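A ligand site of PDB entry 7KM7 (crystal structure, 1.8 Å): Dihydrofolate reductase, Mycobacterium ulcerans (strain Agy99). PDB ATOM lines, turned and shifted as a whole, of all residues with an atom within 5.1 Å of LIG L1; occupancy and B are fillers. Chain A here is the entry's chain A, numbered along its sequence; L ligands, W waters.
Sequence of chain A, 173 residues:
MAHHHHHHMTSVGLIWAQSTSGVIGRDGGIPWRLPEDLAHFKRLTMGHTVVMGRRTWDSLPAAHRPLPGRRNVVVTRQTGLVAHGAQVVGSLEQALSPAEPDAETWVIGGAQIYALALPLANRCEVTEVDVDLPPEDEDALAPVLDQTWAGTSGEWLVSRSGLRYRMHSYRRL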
ATOM      1  N   ILE A  15      26.235  -9.911  12.391  1.00  0.00           N
ATOM      2  CA  ILE A  15      25.535  -8.680  12.018  1.00  0.00           C
ATOM      3  C   ILE A  15      26.263  -7.510  12.662  1.00  0.00           C
ATOM      4  O   ILE A  15      26.617  -7.573  13.843  1.00  0.00           O
ATOM      5  CB  ILE A  15      24.049  -8.745  12.432  1.00  0.00           C
ATOM      6  CG1 ILE A  15      23.329  -7.464  11.992  1.00  0.00           C
ATOM      7  CG2 ILE A  15      23.884  -9.018  13.964  1.00  0.00           C
ATOM      8  CD1 ILE A  15      21.799  -7.586  12.169  1.00  0.00           C
ATOM      9  N   TRP A  16      26.539  -6.454  11.879  1.00  0.00           N
ATOM     10  CA  TRP A  16      27.199  -5.287  12.447  1.00  0.00           C
ATOM     11  C   TRP A  16      26.882  -4.061  11.599  1.00  0.00           C
ATOM     12  O   TRP A  16      26.426  -4.168  10.465  1.00  0.00           O
ATOM     13  CB  TRP A  16      28.728  -5.450  12.532  1.00  0.00           C
ATOM     14  CG  TRP A  16      29.532  -5.435  11.205  1.00  0.00           C
ATOM     15  CD1 TRP A  16      30.008  -4.318  10.515  1.00  0.00           C
ATOM     16  CD2 TRP A  16      30.031  -6.574  10.481  1.00  0.00           C
ATOM     17  NE1 TRP A  16      30.720  -4.720   9.405  1.00  0.00           N
ATOM     18  CE2 TRP A  16      30.753  -6.092   9.363  1.00  0.00           C
ATOM     19  CE3 TRP A  16      29.917  -7.954  10.667  1.00  0.00           C
ATOM     20  CZ2 TRP A  16      31.356  -6.949   8.441  1.00  0.00           C
ATOM     21  CZ3 TRP A  16      30.507  -8.806   9.746  1.00  0.00           C
ATOM     22  CH2 TRP A  16      31.226  -8.297   8.635  1.00  0.00           C
ATOM     23  N   ALA A  17      27.125  -2.901  12.189  1.00  0.00           N
ATOM     24  CA  ALA A  17      27.025  -1.619  11.494  1.00  0.00           C
ATOM     25  C   ALA A  17      28.389  -0.979  11.540  1.00  0.00           C
ATOM     26  O   ALA A  17      29.016  -0.950  12.599  1.00  0.00           O
ATOM     27  CB  ALA A  17      25.976  -0.714  12.174  1.00  0.00           C
ATOM     28  N   ILE A  30      28.870   3.153  20.254  1.00  0.00           N
ATOM     29  CA  ILE A  30      28.826   3.237  18.788  1.00  0.00           C
ATOM     30  C   ILE A  30      28.815   4.707  18.414  1.00  0.00           C
ATOM     31  O   ILE A  30      27.993   5.458  18.944  1.00  0.00           O
ATOM     32  CB  ILE A  30      27.609   2.499  18.200  1.00  0.00           C
ATOM     33  CG1 ILE A  30      27.632   0.997  18.620  1.00  0.00           C
ATOM     34  CG2 ILE A  30      27.533   2.658  16.684  1.00  0.00           C
ATOM     35  CD1 ILE A  30      26.405   0.216  18.199  1.00  0.00           C
ATOM     36  N   ASP A  37      18.938   1.450  11.363  1.00  0.00           N
ATOM     37  CA  ASP A  37      19.789   0.296  11.651  1.00  0.00           C
ATOM     38  C   ASP A  37      19.335  -0.440  12.893  1.00  0.00           C
ATOM     39  O   ASP A  37      19.355  -1.689  12.941  1.00  0.00           O
ATOM     40  CB  ASP A  37      21.250   0.714  11.844  1.00  0.00           C
ATOM     41  CG  ASP A  37      22.112  -0.449  12.262  1.00  0.00           C
ATOM     42  OD1 ASP A  37      22.324  -1.345  11.421  1.00  0.00           O
ATOM     43  OD2 ASP A  37      22.578  -0.464  13.420  1.00  0.00           O
ATOM     44  N   LEU A  38      18.931   0.294  13.938  1.00  0.00           N
ATOM     45  CA  LEU A  38      18.436  -0.404  15.122  1.00  0.00           C
ATOM     46  C   LEU A  38      17.198  -1.219  14.776  1.00  0.00           C
ATOM     47  O   LEU A  38      17.040  -2.359  15.247  1.00  0.00           O
ATOM     48  CB  LEU A  38      18.149   0.573  16.254  1.00  0.00           C
ATOM     49  CG  LEU A  38      19.378   0.744  17.188  1.00  0.00           C
ATOM     50  CD1 LEU A  38      20.644   1.251  16.419  1.00  0.00           C
ATOM     51  CD2 LEU A  38      19.050   1.657  18.349  1.00  0.00           C
ATOM     52  N   ALA A  39      16.328  -0.687  13.911  1.00  0.00           N
ATOM     53  CA  ALA A  39      15.152  -1.441  13.494  1.00  0.00           C
ATOM     54  C   ALA A  39      15.531  -2.670  12.686  1.00  0.00           C
ATOM     55  O   ALA A  39      14.930  -3.731  12.852  1.00  0.00           O
ATOM     56  CB  ALA A  39      14.208  -0.549  12.674  1.00  0.00           C
ATOM     57  N   HIS A  40      16.510  -2.512  11.794  1.00  0.00           N
ATOM     58  CA  HIS A  40      17.033  -3.627  11.011  1.00  0.00           C
ATOM     59  C   HIS A  40      17.638  -4.706  11.913  1.00  0.00           C
ATOM     60  O   HIS A  40      17.376  -5.906  11.742  1.00  0.00           O
ATOM     61  CB  HIS A  40      18.062  -3.057  10.047  1.00  0.00           C
ATOM     62  CG  HIS A  40      18.882  -4.057   9.305  1.00  0.00           C
ATOM     63  ND1 HIS A  40      18.434  -4.680   8.160  1.00  0.00           N
ATOM     64  CD2 HIS A  40      20.161  -4.471   9.485  1.00  0.00           C
ATOM     65  CE1 HIS A  40      19.394  -5.456   7.680  1.00  0.00           C
ATOM     66  NE2 HIS A  40      20.441  -5.352   8.467  1.00  0.00           N
ATOM     67  N   PHE A  41      18.460  -4.285  12.880  1.00  0.00           N
ATOM     68  CA  PHE A  41      19.085  -5.218  13.820  1.00  0.00           C
ATOM     69  C   PHE A  41      18.040  -5.985  14.625  1.00  0.00           C
ATOM     70  O   PHE A  41      18.138  -7.212  14.803  1.00  0.00           O
ATOM     71  CB  PHE A  41      20.022  -4.453  14.756  1.00  0.00           C
ATOM     72  CG  PHE A  41      20.545  -5.253  15.914  1.00  0.00           C
ATOM     73  CD1 PHE A  41      21.655  -6.074  15.754  1.00  0.00           C
ATOM     74  CD2 PHE A  41      19.954  -5.157  17.162  1.00  0.00           C
ATOM     75  CE1 PHE A  41      22.156  -6.824  16.816  1.00  0.00           C
ATOM     76  CE2 PHE A  41      20.445  -5.897  18.239  1.00  0.00           C
ATOM     77  CZ  PHE A  41      21.571  -6.733  18.058  1.00  0.00           C
ATOM     78  N   LYS A  42      17.041  -5.268  15.147  1.00  0.00           N
ATOM     79  CA  LYS A  42      16.007  -5.938  15.948  1.00  0.00           C
ATOM     80  C   LYS A  42      15.238  -6.932  15.101  1.00  0.00           C
ATOM     81  O   LYS A  42      14.977  -8.055  15.540  1.00  0.00           O
ATOM     82  CB  LYS A  42      15.073  -4.903  16.579  1.00  0.00           C
ATOM     83  CG  LYS A  42      14.079  -5.453  17.597  1.00  0.00           C
ATOM     84  CD  LYS A  42      13.120  -4.327  18.029  1.00  0.00           C
ATOM     85  CE  LYS A  42      12.164  -4.741  19.108  1.00  0.00           C
ATOM     86  NZ  LYS A  42      11.250  -3.598  19.373  1.00  0.00           N
ATOM     87  N   THR A  45      17.353 -10.139  14.383  1.00  0.00           N
ATOM     88  CA  THR A  45      17.751 -10.957  15.518  1.00  0.00           C
ATOM     89  C   THR A  45      16.584 -11.457  16.371  1.00  0.00           C
ATOM     90  O   THR A  45      16.770 -12.422  17.134  1.00  0.00           O
ATOM     91  CB  THR A  45      18.737 -10.200  16.425  1.00  0.00           C
ATOM     92  OG1 THR A  45      18.163  -8.972  16.899  1.00  0.00           O
ATOM     93  CG2 THR A  45      20.073  -9.896  15.710  1.00  0.00           C
ATOM     94  N   THR A  56      30.562  -5.731  24.765  1.00  0.00           N
ATOM     95  CA  THR A  56      29.351  -5.331  24.055  1.00  0.00           C
ATOM     96  C   THR A  56      28.125  -5.454  24.953  1.00  0.00           C
ATOM     97  O   THR A  56      27.226  -4.603  24.919  1.00  0.00           O
ATOM     98  CB  THR A  56      29.207  -6.165  22.784  1.00  0.00           C
ATOM     99  OG1 THR A  56      30.232  -5.788  21.855  1.00  0.00           O
ATOM    100  CG2 THR A  56      27.841  -5.971  22.150  1.00  0.00           C
ATOM    101  N   SER A  59      28.040  -2.449  26.886  1.00  0.00           N
ATOM    102  CA  SER A  59      27.728  -1.304  26.042  1.00  0.00           C
ATOM    103  C   SER A  59      26.237  -1.156  25.765  1.00  0.00           C
ATOM    104  O   SER A  59      25.823  -0.107  25.260  1.00  0.00           O
ATOM    105  CB  SER A  59      28.473  -1.388  24.699  1.00  0.00           C
ATOM    106  OG  SER A  59      27.819  -2.248  23.786  1.00  0.00           O
ATOM    107  N   LEU A  60      25.435  -2.177  26.054  1.00  0.00           N
ATOM    108  CA  LEU A  60      23.993  -2.081  25.808  1.00  0.00           C
ATOM    109  C   LEU A  60      23.366  -1.069  26.773  1.00  0.00           C
ATOM    110  O   LEU A  60      23.640  -1.126  27.975  1.00  0.00           O
ATOM    111  CB  LEU A  60      23.315  -3.446  25.976  1.00  0.00           C
ATOM    112  CG  LEU A  60      23.752  -4.559  25.028  1.00  0.00           C
ATOM    113  CD1 LEU A  60      23.076  -5.872  25.406  1.00  0.00           C
ATOM    114  CD2 LEU A  60      23.374  -4.217  23.600  1.00  0.00           C
ATOM    115  N   PRO A  61      22.547  -0.139  26.281  1.00  0.00           N
ATOM    116  CA  PRO A  61      21.818   0.747  27.202  1.00  0.00           C
ATOM    117  C   PRO A  61      20.968  -0.066  28.144  1.00  0.00           C
ATOM    118  O   PRO A  61      20.318  -1.030  27.742  1.00  0.00           O
ATOM    119  CB  PRO A  61      20.939   1.589  26.265  1.00  0.00           C
ATOM    120  CG  PRO A  61      21.552   1.435  24.903  1.00  0.00           C
ATOM    121  CD  PRO A  61      22.148   0.062  24.882  1.00  0.00           C
ATOM    122  N   HIS A  64      17.626  -1.642  27.540  1.00  0.00           N
ATOM    123  CA  HIS A  64      17.622  -2.661  26.493  1.00  0.00           C
ATOM    124  C   HIS A  64      18.537  -3.834  26.829  1.00  0.00           C
ATOM    125  O   HIS A  64      18.969  -4.551  25.909  1.00  0.00           O
ATOM    126  CB  HIS A  64      18.029  -2.061  25.154  1.00  0.00           C
ATOM    127  CG  HIS A  64      17.254  -0.828  24.795  1.00  0.00           C
ATOM    128  ND1 HIS A  64      15.895  -0.847  24.578  1.00  0.00           N
ATOM    129  CD2 HIS A  64      17.649   0.466  24.651  1.00  0.00           C
ATOM    130  CE1 HIS A  64      15.482   0.379  24.280  1.00  0.00           C
ATOM    131  NE2 HIS A  64      16.514   1.195  24.339  1.00  0.00           N
ATOM    132  N   LEU A  67      18.745  -7.913  25.806  1.00  0.00           N
ATOM    133  CA  LEU A  67      17.935  -7.600  24.638  1.00  0.00           C
ATOM    134  C   LEU A  67      16.637  -8.402  24.685  1.00  0.00           C
ATOM    135  O   LEU A  67      16.684  -9.649  24.766  1.00  0.00           O
ATOM    136  CB  LEU A  67      18.714  -7.897  23.344  1.00  0.00           C
ATOM    137  CG  LEU A  67      19.922  -6.980  23.147  1.00  0.00           C
ATOM    138  CD1 LEU A  67      20.858  -7.526  22.050  1.00  0.00           C
ATOM    139  CD2 LEU A  67      19.383  -5.610  22.765  1.00  0.00           C
ATOM    140  N   PRO A  68      15.482  -7.754  24.662  1.00  0.00           N
ATOM    141  CA  PRO A  68      14.219  -8.477  24.881  1.00  0.00           C
ATOM    142  C   PRO A  68      13.868  -9.392  23.715  1.00  0.00           C
ATOM    143  O   PRO A  68      14.162  -9.113  22.550  1.00  0.00           O
ATOM    144  CB  PRO A  68      13.192  -7.353  25.045  1.00  0.00           C
ATOM    145  CG  PRO A  68      13.816  -6.160  24.323  1.00  0.00           C
ATOM    146  CD  PRO A  68      15.283  -6.285  24.552  1.00  0.00           C
ATOM    147  N   ARG A  70      15.034 -12.306  22.907  1.00  0.00           N
ATOM    148  CA  ARG A  70      16.144 -13.085  22.370  1.00  0.00           C
ATOM    149  C   ARG A  70      16.912 -13.709  23.528  1.00  0.00           C
ATOM    150  O   ARG A  70      17.047 -13.087  24.583  1.00  0.00           O
ATOM    151  CB  ARG A  70      17.092 -12.198  21.536  1.00  0.00           C
ATOM    152  CG  ARG A  70      16.512 -11.727  20.195  1.00  0.00           C
ATOM    153  CD  ARG A  70      17.011 -10.322  19.805  1.00  0.00           C
ATOM    154  NE  ARG A  70      16.357  -9.282  20.585  1.00  0.00           N
ATOM    155  CZ  ARG A  70      16.505  -7.981  20.381  1.00  0.00           C
ATOM    156  NH1 ARG A  70      17.325  -7.524  19.442  1.00  0.00           N
ATOM    157  NH2 ARG A  70      15.826  -7.119  21.126  1.00  0.00           N
ATOM    158  N   ILE A 108      26.634 -10.669  17.545  1.00  0.00           N
ATOM    159  CA  ILE A 108      26.286  -9.246  17.456  1.00  0.00           C
ATOM    160  C   ILE A 108      27.434  -8.346  17.890  1.00  0.00           C
ATOM    161  O   ILE A 108      27.220  -7.146  18.092  1.00  0.00           O
ATOM    162  CB  ILE A 108      25.001  -8.938  18.245  1.00  0.00           C
ATOM    163  CG1 ILE A 108      25.190  -9.102  19.748  1.00  0.00           C
ATOM    164  CG2 ILE A 108      23.837  -9.815  17.738  1.00  0.00           C
ATOM    165  CD1 ILE A 108      24.137  -8.383  20.560  1.00  0.00           C
ATOM    166  N   GLY A 109      28.649  -8.886  18.010  1.00  0.00           N
ATOM    167  CA  GLY A 109      29.843  -8.094  18.311  1.00  0.00           C
ATOM    168  C   GLY A 109      30.387  -8.405  19.697  1.00  0.00           C
ATOM    169  O   GLY A 109      29.843  -9.219  20.436  1.00  0.00           O
ATOM    170  N   TYR A 114      33.632 -10.937  16.801  1.00  0.00           N
ATOM    171  CA  TYR A 114      33.517 -11.142  15.346  1.00  0.00           C
ATOM    172  C   TYR A 114      34.704 -11.924  14.824  1.00  0.00           C
ATOM    173  O   TYR A 114      34.551 -12.829  13.989  1.00  0.00           O
ATOM    174  CB  TYR A 114      33.443  -9.810  14.576  1.00  0.00           C
ATOM    175  CG  TYR A 114      32.173  -9.043  14.784  1.00  0.00           C
ATOM    176  CD1 TYR A 114      30.918  -9.669  14.795  1.00  0.00           C
ATOM    177  CD2 TYR A 114      32.205  -7.661  14.970  1.00  0.00           C
ATOM    178  CE1 TYR A 114      29.745  -8.942  14.976  1.00  0.00           C
ATOM    179  CE2 TYR A 114      31.057  -6.931  15.152  1.00  0.00           C
ATOM    180  CZ  TYR A 114      29.825  -7.573  15.149  1.00  0.00           C
ATOM    181  OH  TYR A 114      28.704  -6.818  15.363  1.00  0.00           O
ATOM    182  N   THR A 127      25.433  -3.099   7.891  1.00  0.00           N
ATOM    183  CA  THR A 127      24.948  -1.769   7.579  1.00  0.00           C
ATOM    184  C   THR A 127      26.172  -0.876   7.425  1.00  0.00           C
ATOM    185  O   THR A 127      27.023  -0.809   8.322  1.00  0.00           O
ATOM    186  CB  THR A 127      24.037  -1.221   8.679  1.00  0.00           C
ATOM    187  OG1 THR A 127      22.944  -2.141   8.923  1.00  0.00           O
ATOM    188  CG2 THR A 127      23.473   0.169   8.264  1.00  0.00           C
HETATM  189  C1  LIG L   1      24.651  -3.725  16.349  1.00  0.00           C
HETATM  190  O1  LIG L   1      25.157  -3.719  17.651  1.00  0.00           O
HETATM  191  C2  LIG L   1      22.205  -1.678  17.177  1.00  0.00           C
HETATM  192  C3  LIG L   1      23.627  -1.456  16.602  1.00  0.00           C
HETATM  193  C4  LIG L   1      23.961  -2.685  15.802  1.00  0.00           C
HETATM  194  C5  LIG L   1      23.795  -3.771  13.787  1.00  0.00           C
HETATM  195  C6  LIG L   1      24.920  -4.828  15.483  1.00  0.00           C
HETATM  196  C7  LIG L   1      24.457  -4.549  18.646  1.00  0.00           C
HETATM  197  C8  LIG L   1      24.964  -4.081  20.006  1.00  0.00           C
HETATM  198  C9  LIG L   1      24.271  -2.781  20.396  1.00  0.00           C
HETATM  199  C10 LIG L   1      21.934  -2.156  20.828  1.00  0.00           C
HETATM  200  C11 LIG L   1      22.233  -0.846  21.107  1.00  0.00           C
HETATM  201  C12 LIG L   1      21.229   0.036  21.491  1.00  0.00           C
HETATM  202  C13 LIG L   1      19.911  -0.370  21.585  1.00  0.00           C
HETATM  203  C14 LIG L   1      19.583  -1.709  21.291  1.00  0.00           C
HETATM  204  C15 LIG L   1      18.149  -2.226  21.391  1.00  0.00           C
HETATM  205  C16 LIG L   1      17.518  -2.567  20.020  1.00  0.00           C
HETATM  206  C17 LIG L   1      16.377  -1.612  19.800  1.00  0.00           C
HETATM  207  C18 LIG L   1      16.944  -4.027  20.003  1.00  0.00           C
HETATM  208  C19 LIG L   1      20.604  -2.588  20.902  1.00  0.00           C
HETATM  209  F1  LIG L   1      16.774  -0.276  19.817  1.00  0.00           F
HETATM  210  F2  LIG L   1      15.797  -1.889  18.580  1.00  0.00           F
HETATM  211  N1  LIG L   1      23.518  -2.691  14.534  1.00  0.00           N
HETATM  212  N2  LIG L   1      23.339  -3.771  12.518  1.00  0.00           N
HETATM  213  N3  LIG L   1      24.476  -4.838  14.231  1.00  0.00           N
HETATM  214  N4  LIG L   1      25.622  -5.883  15.949  1.00  0.00           N
HETATM  215  O2  LIG L   1      22.867  -3.095  20.430  1.00  0.00           O
HETATM  216  O3  LIG L   1      15.994  -4.215  20.794  1.00  0.00           O
HETATM  217  O4  LIG L   1      17.497  -4.799  19.183  1.00  0.00           O
HETATM  218  P1  LG2 L   2      33.905  -7.330  22.601  1.00  0.00           P
HETATM  219  O1  LG2 L   2      34.252  -8.276  21.493  1.00  0.00           O
HETATM  220  O2  LG2 L   2      32.390  -7.034  22.574  1.00  0.00           O
HETATM  221  O3  LG2 L   2      34.222  -8.048  24.036  1.00  0.00           O
HETATM  222  C1  LG2 L   2      35.578  -8.310  24.438  1.00  0.00           C
HETATM  223  C2  LG2 L   2      35.551  -9.245  25.626  1.00  0.00           C
HETATM  224  O4  LG2 L   2      35.101 -10.552  25.231  1.00  0.00           O
HETATM  225  C3  LG2 L   2      36.918  -9.470  26.240  1.00  0.00           C
HETATM  226  O5  LG2 L   2      37.289  -8.314  26.974  1.00  0.00           O
HETATM  227  C4  LG2 L   2      36.616 -10.748  27.020  1.00  0.00           C
HETATM  228  O6  LG2 L   2      35.775 -10.488  28.163  1.00  0.00           O
HETATM  229  C5  LG2 L   2      35.768 -11.530  26.019  1.00  0.00           C
HETATM  230  N1  LG2 L   2      36.562 -12.416  25.161  1.00  0.00           N
HETATM  231  C6  LG2 L   2      37.316 -12.076  24.069  1.00  0.00           C
HETATM  232  N2  LG2 L   2      37.909 -13.087  23.496  1.00  0.00           N
HETATM  233  C7  LG2 L   2      37.534 -14.175  24.272  1.00  0.00           C
HETATM  234  C8  LG2 L   2      37.852 -15.544  24.212  1.00  0.00           C
HETATM  235  N3  LG2 L   2      38.634 -16.089  23.273  1.00  0.00           N
HETATM  236  N4  LG2 L   2      37.327 -16.353  25.150  1.00  0.00           N
HETATM  237  C9  LG2 L   2      36.534 -15.816  26.087  1.00  0.00           C
HETATM  238  N5  LG2 L   2      36.163 -14.545  26.250  1.00  0.00           N
HETATM  239  C10 LG2 L   2      36.696 -13.768  25.298  1.00  0.00           C
HETATM  240  O7  LG2 L   2      34.792  -6.026  22.662  1.00  0.00           O
HETATM  241  P2  LG2 L   2      35.317  -4.935  21.622  1.00  0.00           P
HETATM  242  O8  LG2 L   2      36.019  -5.649  20.528  1.00  0.00           O
HETATM  243  O9  LG2 L   2      36.025  -3.874  22.375  1.00  0.00           O
HETATM  244  O10 LG2 L   2      33.954  -4.396  21.016  1.00  0.00           O
HETATM  245  C11 LG2 L   2      33.134  -3.508  21.795  1.00  0.00           C
HETATM  246  C12 LG2 L   2      32.961  -2.226  21.030  1.00  0.00           C
HETATM  247  O11 LG2 L   2      32.266  -2.480  19.779  1.00  0.00           O
HETATM  248  C13 LG2 L   2      32.121  -1.162  21.739  1.00  0.00           C
HETATM  249  O12 LG2 L   2      32.547   0.127  21.334  1.00  0.00           O
HETATM  250  C14 LG2 L   2      30.723  -1.468  21.209  1.00  0.00           C
HETATM  251  O13 LG2 L   2      29.842  -0.361  21.366  1.00  0.00           O
HETATM  252  C15 LG2 L   2      31.066  -1.756  19.754  1.00  0.00           C
HETATM  253  N6  LG2 L   2      30.017  -2.587  18.997  1.00  0.00           N
HETATM  254  C16 LG2 L   2      29.595  -2.104  17.812  1.00  0.00           C
HETATM  255  C17 LG2 L   2      28.783  -2.879  17.006  1.00  0.00           C
HETATM  256  C18 LG2 L   2      28.273  -2.354  15.695  1.00  0.00           C
HETATM  257  O14 LG2 L   2      27.656  -3.113  14.953  1.00  0.00           O
HETATM  258  N7  LG2 L   2      28.562  -1.071  15.364  1.00  0.00           N
HETATM  259  C19 LG2 L   2      28.392  -4.148  17.466  1.00  0.00           C
HETATM  260  C20 LG2 L   2      28.820  -4.585  18.711  1.00  0.00           C
HETATM  261  C21 LG2 L   2      29.617  -3.788  19.474  1.00  0.00           C
HETATM  262  P3  LG2 L   2      36.353 -10.186  29.611  1.00  0.00           P
HETATM  263  O15 LG2 L   2      35.147 -10.051  30.510  1.00  0.00           O
HETATM  264  O16 LG2 L   2      37.198 -11.420  29.980  1.00  0.00           O
HETATM  265  O17 LG2 L   2      37.193  -8.956  29.502  1.00  0.00           O
HETATM  266  O   HOH W   1      13.940  -0.429  16.489  1.00  0.00           O
HETATM  267  O   HOH W   2      25.303   0.285  22.101  1.00  0.00           O
HETATM  268  O   HOH W   3      23.298  -4.929   9.609  1.00  0.00           O
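Trp 16 touches LIG L1 (CA to N3, 3.3 Å).
Ala 17 touches LIG L1.
Ile 30 touches LIG L1 (CD1 to C3, 3.6 Å).
Leu 38 touches LIG L1 (CD2 to F1, 3.3 Å).
CD2 of Phe 41 touches O4 of LIG L1, 3.2 Å away.
Lys 42 touches LIG L1.
Leu 60 touches LIG L1.
Pro 61 touches LIG L1 (CD to C12, 3.5 Å).
CB of His 64 touches C15 of LIG L1, 3.8 Å away.
CD2 of Leu 67 touches C19 of LIG L1 (3.8 Å).
Thr 127 touches LIG L1 (OG1 to N2, 3.97 Å).
Hydrophobic or aromatic side chains within 4 Å of LIG L1: Ile 15, Ala 17, Ile 30, Leu 38, Phe 41, Leu 60, Pro 61, His 64, Leu 67 and Ile 108.
The nearest printed residue that does not touch LIG L1 is Thr 56 (4.1 Å).
The backbone NH of Thr 56 is in hydrogen-bond range of an oxygen (O2) of LG2 L2 (3.1 Å).
The side-chain hydroxyl (OG1) of Thr 56 lies within hydrogen-bond range of an oxygen (O2) of LG2 L2.
O of Ala 17 is in hydrogen-bond range of N7 of LG2 L2 (2.8 Å).
O of Ile 108 sits at hydrogen-bond distance from N4 of LIG L1.
OD2 of Asp 37 sits at hydrogen-bond distance from N1 of LIG L1.
N4 of LIG L1 sits at hydrogen-bond distance from OH of Tyr 114, at 3.3 Å.
The backbone NH (N) of Ala 17 is in hydrogen-bond range of an oxygen (O14) of LG2 L2 (2.8 Å).
O of Ile 15 is in hydrogen-bond range of N4 of LIG L1, at 2.9 Å.
The guanidinium group (NH1) of Arg 70 is in salt-bridge range of an oxygen (O4) of LIG L1 (2.7 Å).
The backbone carbonyl oxygen (O) of Ile 108 is in hydrogen-bond range of the side-chain hydroxyl (OH) of Tyr 114, at 3.1 Å.
The backbone carbonyl oxygen (O) of Trp 16 is in hydrogen-bond range of the backbone NH (N) of Thr 127 (3.0 Å).
The backbone carbonyl oxygen (O) of Ile 15 is in hydrogen-bond range of the side-chain hydroxyl (OH) of Tyr 114 (2.7 Å).
The side-chain hydroxyl (OH) of Tyr 114 sits close to the backbone NH (N) of Gly 109 (3.4 Å).
NE of Arg 70 sits at hydrogen-bond distance from O of Pro 68.
NH1 of Arg 70 sits at hydrogen-bond distance from OG1 of Thr 45, at 3.0 Å.
The side-chain hydroxyl (OG1) of Thr 127 is in hydrogen-bond range of the side-chain carboxylate (OD1) of Asp 37 (2.7 Å).
O of Phe 41 sits at hydrogen-bond distance from OG1 of Thr 45, 2.7 Å away.
Water W3 lies within hydrogen-bond range of OG1 of Thr 127 (2.9 Å), NE2 of His 40 (3.1 Å), N2 of LIG L1 (3.1 Å) and O of Trp 16 (3.3 Å).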
